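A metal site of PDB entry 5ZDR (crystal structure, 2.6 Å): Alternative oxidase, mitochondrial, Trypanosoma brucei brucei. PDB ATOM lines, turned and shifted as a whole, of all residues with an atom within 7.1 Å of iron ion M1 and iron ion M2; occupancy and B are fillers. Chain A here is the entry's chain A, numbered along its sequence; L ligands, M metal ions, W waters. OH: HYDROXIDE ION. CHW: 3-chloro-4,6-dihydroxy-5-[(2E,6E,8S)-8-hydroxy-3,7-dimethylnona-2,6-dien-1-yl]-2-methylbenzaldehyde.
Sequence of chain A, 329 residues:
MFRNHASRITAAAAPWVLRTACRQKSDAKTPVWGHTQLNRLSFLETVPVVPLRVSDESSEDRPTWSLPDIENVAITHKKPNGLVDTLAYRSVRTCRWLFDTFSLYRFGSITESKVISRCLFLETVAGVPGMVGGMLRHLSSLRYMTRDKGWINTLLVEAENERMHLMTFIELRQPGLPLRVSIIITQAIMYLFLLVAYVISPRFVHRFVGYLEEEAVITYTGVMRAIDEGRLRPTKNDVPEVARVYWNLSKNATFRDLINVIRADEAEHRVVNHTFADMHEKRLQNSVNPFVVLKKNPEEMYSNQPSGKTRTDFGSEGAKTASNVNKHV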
ATOM      1  N   CYS A 119      -2.145  23.857 -27.888  1.00  0.00           N
ATOM      2  CA  CYS A 119      -2.573  22.457 -28.013  1.00  0.00           C
ATOM      3  C   CYS A 119      -2.109  21.835 -29.357  1.00  0.00           C
ATOM      4  O   CYS A 119      -1.522  20.751 -29.390  1.00  0.00           O
ATOM      5  CB  CYS A 119      -4.083  22.361 -27.862  1.00  0.00           C
ATOM      6  SG  CYS A 119      -4.786  23.368 -26.512  1.00  0.00           S
ATOM      7  N   LEU A 122       1.918  21.184 -29.152  1.00  0.00           N
ATOM      8  CA  LEU A 122       2.190  20.156 -28.182  1.00  0.00           C
ATOM      9  C   LEU A 122       1.596  18.836 -28.591  1.00  0.00           C
ATOM     10  O   LEU A 122       2.225  17.800 -28.399  1.00  0.00           O
ATOM     11  CB  LEU A 122       1.643  20.580 -26.821  1.00  0.00           C
ATOM     12  CG  LEU A 122       2.467  21.649 -26.093  1.00  0.00           C
ATOM     13  CD1 LEU A 122       1.771  22.000 -24.819  1.00  0.00           C
ATOM     14  CD2 LEU A 122       3.883  21.193 -25.766  1.00  0.00           C
ATOM     15  N   GLU A 123       0.392  18.826 -29.149  1.00  0.00           N
ATOM     16  CA  GLU A 123      -0.176  17.550 -29.593  1.00  0.00           C
ATOM     17  C   GLU A 123       0.713  16.877 -30.642  1.00  0.00           C
ATOM     18  O   GLU A 123       0.748  15.660 -30.690  1.00  0.00           O
ATOM     19  CB  GLU A 123      -1.634  17.680 -30.040  1.00  0.00           C
ATOM     20  CG  GLU A 123      -2.632  17.911 -28.878  1.00  0.00           C
ATOM     21  CD  GLU A 123      -2.766  16.750 -27.862  1.00  0.00           C
ATOM     22  OE1 GLU A 123      -3.717  16.787 -27.055  1.00  0.00           O
ATOM     23  OE2 GLU A 123      -1.939  15.803 -27.829  1.00  0.00           O
ATOM     24  N   ALA A 126       2.938  14.617 -28.377  1.00  0.00           N
ATOM     25  CA  ALA A 126       2.219  13.620 -27.570  1.00  0.00           C
ATOM     26  C   ALA A 126       1.951  12.323 -28.365  1.00  0.00           C
ATOM     27  O   ALA A 126       1.771  11.232 -27.792  1.00  0.00           O
ATOM     28  CB  ALA A 126       0.906  14.215 -27.079  1.00  0.00           C
ATOM     29  N   GLY A 127       1.915  12.466 -29.685  1.00  0.00           N
ATOM     30  CA  GLY A 127       1.790  11.313 -30.548  1.00  0.00           C
ATOM     31  C   GLY A 127       2.991  10.397 -30.643  1.00  0.00           C
ATOM     32  O   GLY A 127       2.853   9.298 -31.186  1.00  0.00           O
ATOM     33  N   GLU A 158      -3.203   4.961 -28.150  1.00  0.00           N
ATOM     34  CA  GLU A 158      -2.855   6.237 -27.490  1.00  0.00           C
ATOM     35  C   GLU A 158      -2.233   7.111 -28.544  1.00  0.00           C
ATOM     36  O   GLU A 158      -2.790   8.146 -28.882  1.00  0.00           O
ATOM     37  CB  GLU A 158      -1.849   6.056 -26.316  1.00  0.00           C
ATOM     38  CG  GLU A 158      -1.686   7.297 -25.410  1.00  0.00           C
ATOM     39  CD  GLU A 158      -0.250   7.551 -24.892  1.00  0.00           C
ATOM     40  OE1 GLU A 158      -0.051   7.619 -23.655  1.00  0.00           O
ATOM     41  OE2 GLU A 158       0.692   7.708 -25.709  1.00  0.00           O
ATOM     42  N   ASN A 161      -4.909   8.128 -30.771  1.00  0.00           N
ATOM     43  CA  ASN A 161      -5.817   8.995 -30.062  1.00  0.00           C
ATOM     44  C   ASN A 161      -5.242  10.397 -29.846  1.00  0.00           C
ATOM     45  O   ASN A 161      -5.989  11.384 -29.837  1.00  0.00           O
ATOM     46  CB  ASN A 161      -6.149   8.294 -28.736  1.00  0.00           C
ATOM     47  CG  ASN A 161      -6.996   9.144 -27.809  1.00  0.00           C
ATOM     48  OD1 ASN A 161      -6.539   9.535 -26.737  1.00  0.00           O
ATOM     49  ND2 ASN A 161      -8.220   9.441 -28.221  1.00  0.00           N
ATOM     50  N   GLU A 162      -3.928  10.484 -29.702  1.00  0.00           N
ATOM     51  CA  GLU A 162      -3.228  11.783 -29.660  1.00  0.00           C
ATOM     52  C   GLU A 162      -3.022  12.367 -31.071  1.00  0.00           C
ATOM     53  O   GLU A 162      -3.031  13.594 -31.288  1.00  0.00           O
ATOM     54  CB  GLU A 162      -1.905  11.653 -28.933  1.00  0.00           C
ATOM     55  CG  GLU A 162      -1.993  11.214 -27.477  1.00  0.00           C
ATOM     56  CD  GLU A 162      -2.355  12.341 -26.539  1.00  0.00           C
ATOM     57  OE1 GLU A 162      -3.432  12.952 -26.738  1.00  0.00           O
ATOM     58  OE2 GLU A 162      -1.573  12.599 -25.594  1.00  0.00           O
ATOM     59  N   ARG A 163      -2.853  11.493 -32.050  1.00  0.00           N
ATOM     60  CA  ARG A 163      -2.772  11.980 -33.407  1.00  0.00           C
ATOM     61  C   ARG A 163      -4.123  12.587 -33.747  1.00  0.00           C
ATOM     62  O   ARG A 163      -4.163  13.660 -34.374  1.00  0.00           O
ATOM     63  CB  ARG A 163      -2.358  10.882 -34.401  1.00  0.00           C
ATOM     64  CG  ARG A 163      -2.053  11.442 -35.778  1.00  0.00           C
ATOM     65  CD  ARG A 163      -1.652  10.395 -36.803  1.00  0.00           C
ATOM     66  NE  ARG A 163      -2.692   9.382 -37.057  1.00  0.00           N
ATOM     67  CZ  ARG A 163      -3.758   9.547 -37.835  1.00  0.00           C
ATOM     68  NH1 ARG A 163      -4.624   8.555 -37.962  1.00  0.00           N
ATOM     69  NH2 ARG A 163      -3.985  10.712 -38.464  1.00  0.00           N
ATOM     70  N   HIS A 165      -5.974  14.132 -31.723  1.00  0.00           N
ATOM     71  CA  HIS A 165      -5.978  15.426 -31.050  1.00  0.00           C
ATOM     72  C   HIS A 165      -5.349  16.515 -31.915  1.00  0.00           C
ATOM     73  O   HIS A 165      -5.864  17.650 -32.011  1.00  0.00           O
ATOM     74  CB  HIS A 165      -5.233  15.278 -29.739  1.00  0.00           C
ATOM     75  CG  HIS A 165      -6.011  14.509 -28.699  1.00  0.00           C
ATOM     76  ND1 HIS A 165      -5.601  14.416 -27.388  1.00  0.00           N
ATOM     77  CD2 HIS A 165      -7.200  13.868 -28.772  1.00  0.00           C
ATOM     78  CE1 HIS A 165      -6.490  13.723 -26.706  1.00  0.00           C
ATOM     79  NE2 HIS A 165      -7.469  13.395 -27.523  1.00  0.00           N
ATOM     80  N   LEU A 166      -4.248  16.178 -32.587  1.00  0.00           N
ATOM     81  CA  LEU A 166      -3.700  17.025 -33.624  1.00  0.00           C
ATOM     82  C   LEU A 166      -4.748  17.280 -34.689  1.00  0.00           C
ATOM     83  O   LEU A 166      -4.965  18.419 -35.067  1.00  0.00           O
ATOM     84  CB  LEU A 166      -2.488  16.384 -34.297  1.00  0.00           C
ATOM     85  CG  LEU A 166      -1.320  17.330 -34.590  1.00  0.00           C
ATOM     86  CD1 LEU A 166      -0.515  16.797 -35.742  1.00  0.00           C
ATOM     87  CD2 LEU A 166      -1.786  18.760 -34.876  1.00  0.00           C
ATOM     88  N   PHE A 169      -7.500  19.907 -33.785  1.00  0.00           N
ATOM     89  CA  PHE A 169      -6.998  21.273 -33.673  1.00  0.00           C
ATOM     90  C   PHE A 169      -6.542  21.872 -35.012  1.00  0.00           C
ATOM     91  O   PHE A 169      -6.664  23.087 -35.230  1.00  0.00           O
ATOM     92  CB  PHE A 169      -5.884  21.361 -32.631  1.00  0.00           C
ATOM     93  CG  PHE A 169      -6.300  20.982 -31.237  1.00  0.00           C
ATOM     94  CD1 PHE A 169      -7.490  21.447 -30.717  1.00  0.00           C
ATOM     95  CD2 PHE A 169      -5.494  20.179 -30.457  1.00  0.00           C
ATOM     96  CE1 PHE A 169      -7.875  21.108 -29.417  1.00  0.00           C
ATOM     97  CE2 PHE A 169      -5.861  19.827 -29.167  1.00  0.00           C
ATOM     98  CZ  PHE A 169      -7.062  20.293 -28.646  1.00  0.00           C
ATOM     99  N   VAL A 209       5.711  10.350 -19.537  1.00  0.00           N
ATOM    100  CA  VAL A 209       4.317  10.578 -20.034  1.00  0.00           C
ATOM    101  C   VAL A 209       3.290  10.632 -18.861  1.00  0.00           C
ATOM    102  O   VAL A 209       2.290  11.395 -18.872  1.00  0.00           O
ATOM    103  CB  VAL A 209       3.885   9.450 -20.987  1.00  0.00           C
ATOM    104  CG1 VAL A 209       2.517   9.731 -21.539  1.00  0.00           C
ATOM    105  CG2 VAL A 209       4.878   9.303 -22.123  1.00  0.00           C
ATOM    106  N   LEU A 212       4.012  14.287 -17.984  1.00  0.00           N
ATOM    107  CA  LEU A 212       3.520  14.983 -19.152  1.00  0.00           C
ATOM    108  C   LEU A 212       1.989  15.159 -19.084  1.00  0.00           C
ATOM    109  O   LEU A 212       1.479  16.280 -19.069  1.00  0.00           O
ATOM    110  CB  LEU A 212       3.885  14.161 -20.388  1.00  0.00           C
ATOM    111  CG  LEU A 212       4.881  14.607 -21.455  1.00  0.00           C
ATOM    112  CD1 LEU A 212       4.195  14.260 -22.754  1.00  0.00           C
ATOM    113  CD2 LEU A 212       5.185  16.093 -21.426  1.00  0.00           C
ATOM    114  N   GLU A 213       1.247  14.047 -19.012  1.00  0.00           N
ATOM    115  CA  GLU A 213      -0.237  14.126 -18.913  1.00  0.00           C
ATOM    116  C   GLU A 213      -0.796  14.809 -17.636  1.00  0.00           C
ATOM    117  O   GLU A 213      -1.901  15.367 -17.649  1.00  0.00           O
ATOM    118  CB  GLU A 213      -0.848  12.716 -19.025  1.00  0.00           C
ATOM    119  CG  GLU A 213      -0.450  11.918 -20.275  1.00  0.00           C
ATOM    120  CD  GLU A 213      -1.029  12.490 -21.530  1.00  0.00           C
ATOM    121  OE1 GLU A 213      -1.020  13.712 -21.617  1.00  0.00           O
ATOM    122  OE2 GLU A 213      -1.504  11.739 -22.410  1.00  0.00           O
ATOM    123  N   ALA A 216      -0.923  18.067 -18.927  1.00  0.00           N
ATOM    124  CA  ALA A 216      -1.988  18.146 -19.941  1.00  0.00           C
ATOM    125  C   ALA A 216      -3.355  18.293 -19.281  1.00  0.00           C
ATOM    126  O   ALA A 216      -4.222  19.010 -19.821  1.00  0.00           O
ATOM    127  CB  ALA A 216      -1.978  16.881 -20.777  1.00  0.00           C
ATOM    128  N   TYR A 220      -5.877  21.774 -19.473  1.00  0.00           N
ATOM    129  CA  TYR A 220      -7.221  21.725 -20.049  1.00  0.00           C
ATOM    130  C   TYR A 220      -8.332  22.065 -19.056  1.00  0.00           C
ATOM    131  O   TYR A 220      -9.315  22.708 -19.464  1.00  0.00           O
ATOM    132  CB  TYR A 220      -7.510  20.377 -20.729  1.00  0.00           C
ATOM    133  CG  TYR A 220      -6.891  20.154 -22.116  1.00  0.00           C
ATOM    134  CD1 TYR A 220      -7.100  21.034 -23.162  1.00  0.00           C
ATOM    135  CD2 TYR A 220      -6.135  19.007 -22.368  1.00  0.00           C
ATOM    136  CE1 TYR A 220      -6.557  20.791 -24.412  1.00  0.00           C
ATOM    137  CE2 TYR A 220      -5.579  18.774 -23.599  1.00  0.00           C
ATOM    138  CZ  TYR A 220      -5.797  19.656 -24.625  1.00  0.00           C
ATOM    139  OH  TYR A 220      -5.240  19.371 -25.873  1.00  0.00           O
ATOM    140  N   ILE A 262     -11.219  15.585 -24.779  1.00  0.00           N
ATOM    141  CA  ILE A 262      -9.738  15.617 -24.904  1.00  0.00           C
ATOM    142  C   ILE A 262      -9.010  15.577 -23.517  1.00  0.00           C
ATOM    143  O   ILE A 262      -7.976  14.969 -23.376  1.00  0.00           O
ATOM    144  CB  ILE A 262      -9.280  16.827 -25.744  1.00  0.00           C
ATOM    145  CG1 ILE A 262      -9.492  16.530 -27.239  1.00  0.00           C
ATOM    146  CG2 ILE A 262      -7.798  17.156 -25.514  1.00  0.00           C
ATOM    147  CD1 ILE A 262      -9.303  17.730 -28.141  1.00  0.00           C
ATOM    148  N   ASP A 265      -9.483  11.709 -22.051  1.00  0.00           N
ATOM    149  CA  ASP A 265      -8.366  10.984 -22.712  1.00  0.00           C
ATOM    150  C   ASP A 265      -6.977  11.135 -22.015  1.00  0.00           C
ATOM    151  O   ASP A 265      -6.160  10.181 -21.970  1.00  0.00           O
ATOM    152  CB  ASP A 265      -8.263  11.451 -24.160  1.00  0.00           C
ATOM    153  CG  ASP A 265      -9.359  10.830 -25.084  1.00  0.00           C
ATOM    154  OD1 ASP A 265     -10.096   9.906 -24.611  1.00  0.00           O
ATOM    155  OD2 ASP A 265      -9.444  11.243 -26.285  1.00  0.00           O
ATOM    156  N   GLU A 266      -6.684  12.302 -21.445  1.00  0.00           N
ATOM    157  CA  GLU A 266      -5.314  12.535 -20.952  1.00  0.00           C
ATOM    158  C   GLU A 266      -5.203  12.020 -19.536  1.00  0.00           C
ATOM    159  O   GLU A 266      -4.141  11.591 -19.075  1.00  0.00           O
ATOM    160  CB  GLU A 266      -4.902  13.993 -21.069  1.00  0.00           C
ATOM    161  CG  GLU A 266      -5.235  14.671 -22.407  1.00  0.00           C
ATOM    162  CD  GLU A 266      -4.244  14.453 -23.549  1.00  0.00           C
ATOM    163  OE1 GLU A 266      -4.591  14.913 -24.684  1.00  0.00           O
ATOM    164  OE2 GLU A 266      -3.130  13.885 -23.376  1.00  0.00           O
ATOM    165  N   HIS A 269      -4.351   8.292 -20.037  1.00  0.00           N
ATOM    166  CA  HIS A 269      -2.963   8.099 -20.415  1.00  0.00           C
ATOM    167  C   HIS A 269      -2.062   8.313 -19.225  1.00  0.00           C
ATOM    168  O   HIS A 269      -1.109   7.561 -19.000  1.00  0.00           O
ATOM    169  CB  HIS A 269      -2.604   9.108 -21.478  1.00  0.00           C
ATOM    170  CG  HIS A 269      -3.427   9.010 -22.720  1.00  0.00           C
ATOM    171  ND1 HIS A 269      -3.514  10.030 -23.643  1.00  0.00           N
ATOM    172  CD2 HIS A 269      -4.205   8.010 -23.204  1.00  0.00           C
ATOM    173  CE1 HIS A 269      -4.298   9.658 -24.642  1.00  0.00           C
ATOM    174  NE2 HIS A 269      -4.724   8.434 -24.396  1.00  0.00           N
ATOM    175  N   ARG A 270      -2.364   9.386 -18.478  1.00  0.00           N
ATOM    176  CA  ARG A 270      -1.755   9.627 -17.149  1.00  0.00           C
ATOM    177  C   ARG A 270      -1.704   8.354 -16.290  1.00  0.00           C
ATOM    178  O   ARG A 270      -0.618   7.994 -15.805  1.00  0.00           O
ATOM    179  CB  ARG A 270      -2.526  10.747 -16.412  1.00  0.00           C
ATOM    180  CG  ARG A 270      -2.028  11.091 -15.020  1.00  0.00           C
ATOM    181  CD  ARG A 270      -2.841  12.242 -14.393  1.00  0.00           C
ATOM    182  NE  ARG A 270      -4.259  11.899 -14.195  1.00  0.00           N
ATOM    183  CZ  ARG A 270      -5.220  12.770 -13.873  1.00  0.00           C
ATOM    184  NH1 ARG A 270      -4.931  14.054 -13.702  1.00  0.00           N
ATOM    185  NH2 ARG A 270      -6.469  12.348 -13.693  1.00  0.00           N
HETATM  186  O    OH L   1      -2.238  15.226 -25.297  1.00  0.00           O
HETATM  187  OAA CHW L   2       2.444  18.270 -21.763  1.00  0.00           O
HETATM  188  CAB CHW L   2       1.382  19.004 -22.221  1.00  0.00           C
HETATM  189  CAC CHW L   2       1.076  20.239 -21.664  1.00  0.00           C
HETATM  190  CAD CHW L   2       1.928  20.799 -20.579  1.00  0.00           C
HETATM  191  CAE CHW L   2       3.184  21.268 -21.264  1.00  0.00           C
HETATM  192  CAF CHW L   2       4.374  20.789 -20.920  1.00  0.00           C
HETATM  193  CAG CHW L   2       5.590  21.272 -21.644  1.00  0.00           C
HETATM  194  CAH CHW L   2       6.012  20.214 -22.630  1.00  0.00           C
HETATM  195  CAI CHW L   2       7.077  20.823 -23.520  1.00  0.00           C
HETATM  196  CAJ CHW L   2       7.744  20.114 -24.442  1.00  0.00           C
HETATM  197  CAK CHW L   2       8.787  20.812 -25.276  1.00  0.00           C
HETATM  198  OAL CHW L   2       9.352  19.848 -26.157  1.00  0.00           O
HETATM  199  OAM CHW L   2       1.914  16.574 -23.091  1.00  0.00           O
HETATM  200  CAN CHW L   2       1.023  17.126 -23.731  1.00  0.00           C
HETATM  201  CAO CHW L   2       0.630  18.472 -23.244  1.00  0.00           C
HETATM  202  CAP CHW L   2       0.033  20.970 -22.132  1.00  0.00           C
HETATM  203  OAQ CHW L   2      -0.228  22.176 -21.586  1.00  0.00           O
HETATM  204  CAR CHW L   2       4.576  19.782 -19.816  1.00  0.00           C
HETATM  205  CAS CHW L   2       7.491  18.638 -24.666  1.00  0.00           C
HETATM  206  CAT CHW L   2       8.179  21.956 -26.088  1.00  0.00           C
HETATM  207  CAU CHW L   2      -0.507  19.257 -23.749  1.00  0.00           C
HETATM  208  CAV CHW L   2      -0.731  20.489 -23.177  1.00  0.00           C
HETATM  209 CLAW CHW L   2      -2.078  21.506 -23.760  1.00  0.00          CL
HETATM  210  CAX CHW L   2      -1.405  18.794 -24.855  1.00  0.00           C
HETATM  211 FE    FE M   1      -1.084  13.623 -23.916  1.00  0.00          FE
HETATM  212 FE    FE M   2      -3.614  14.865 -26.366  1.00  0.00          FE
HETATM  213  O   HOH W   1       1.500  13.340 -23.740  1.00  0.00           O
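The backbone carbonyl oxygen (O) of Leu 212 lies within hydrogen-bond range of an oxygen (OAA) of CHW L2 (3.5 Å).
OH of Tyr 220 sits close to OE1 of Glu 123, at 3.2 Å.
A ring nitrogen (NE2) of His 165 sits close to the backbone carbonyl oxygen (O) of Asn 161, 3.4 Å away.
The side-chain carboxylate of Asp 265 is in hydrogen-bond range of a ring nitrogen (NE2) of His 165, 3.2 Å away.
OE2 of Glu 213 lies close to ND1 of His 269 (2.9 Å).
Ala 126 touches iron ion M1.
Within 4 Å of iron ion M1: Ala 126, Glu 162, Glu 213 and Glu 266.
Along chain A the residues within 4 Å of iron ion M1 span positions 126 to 266.
The nearest printed residue that does not touch iron ion M1 is His 269 (4.3 Å).
Four residues have an atom within 4 Å of iron ion M2: Glu 123, Glu 162, His 165 and Glu 266.
The nearest printed residue that does not touch iron ion M2 is Ala 126 (4.6 Å).
Iron ion M1 is bound by the side-chain carboxylate (OE2) of Glu 162 (2.0 Å), the side-chain carboxylate (OE2) of Glu 266 (2.1 Å), the side-chain carboxylate (OE1) of Glu 213 (2.3 Å), an oxygen (O) of OH L1 (2.4 Å) and the side-chain carboxylate (OE2) of Glu 213 (2.4 Å).
Iron ion M1 has five donor atoms within binding distance.
Slightly farther from iron ion M1 lies water W1 (2.6 Å).
Iron ion M2 is bound by O of OH L1 (1.8 Å), OE1 of Glu 266 (1.9 Å), OE1 of Glu 162 (2.0 Å), OE1 of Glu 123 (2.0 Å), ND1 of His 165 (2.3 Å) and OE2 of Glu 123 (2.4 Å).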
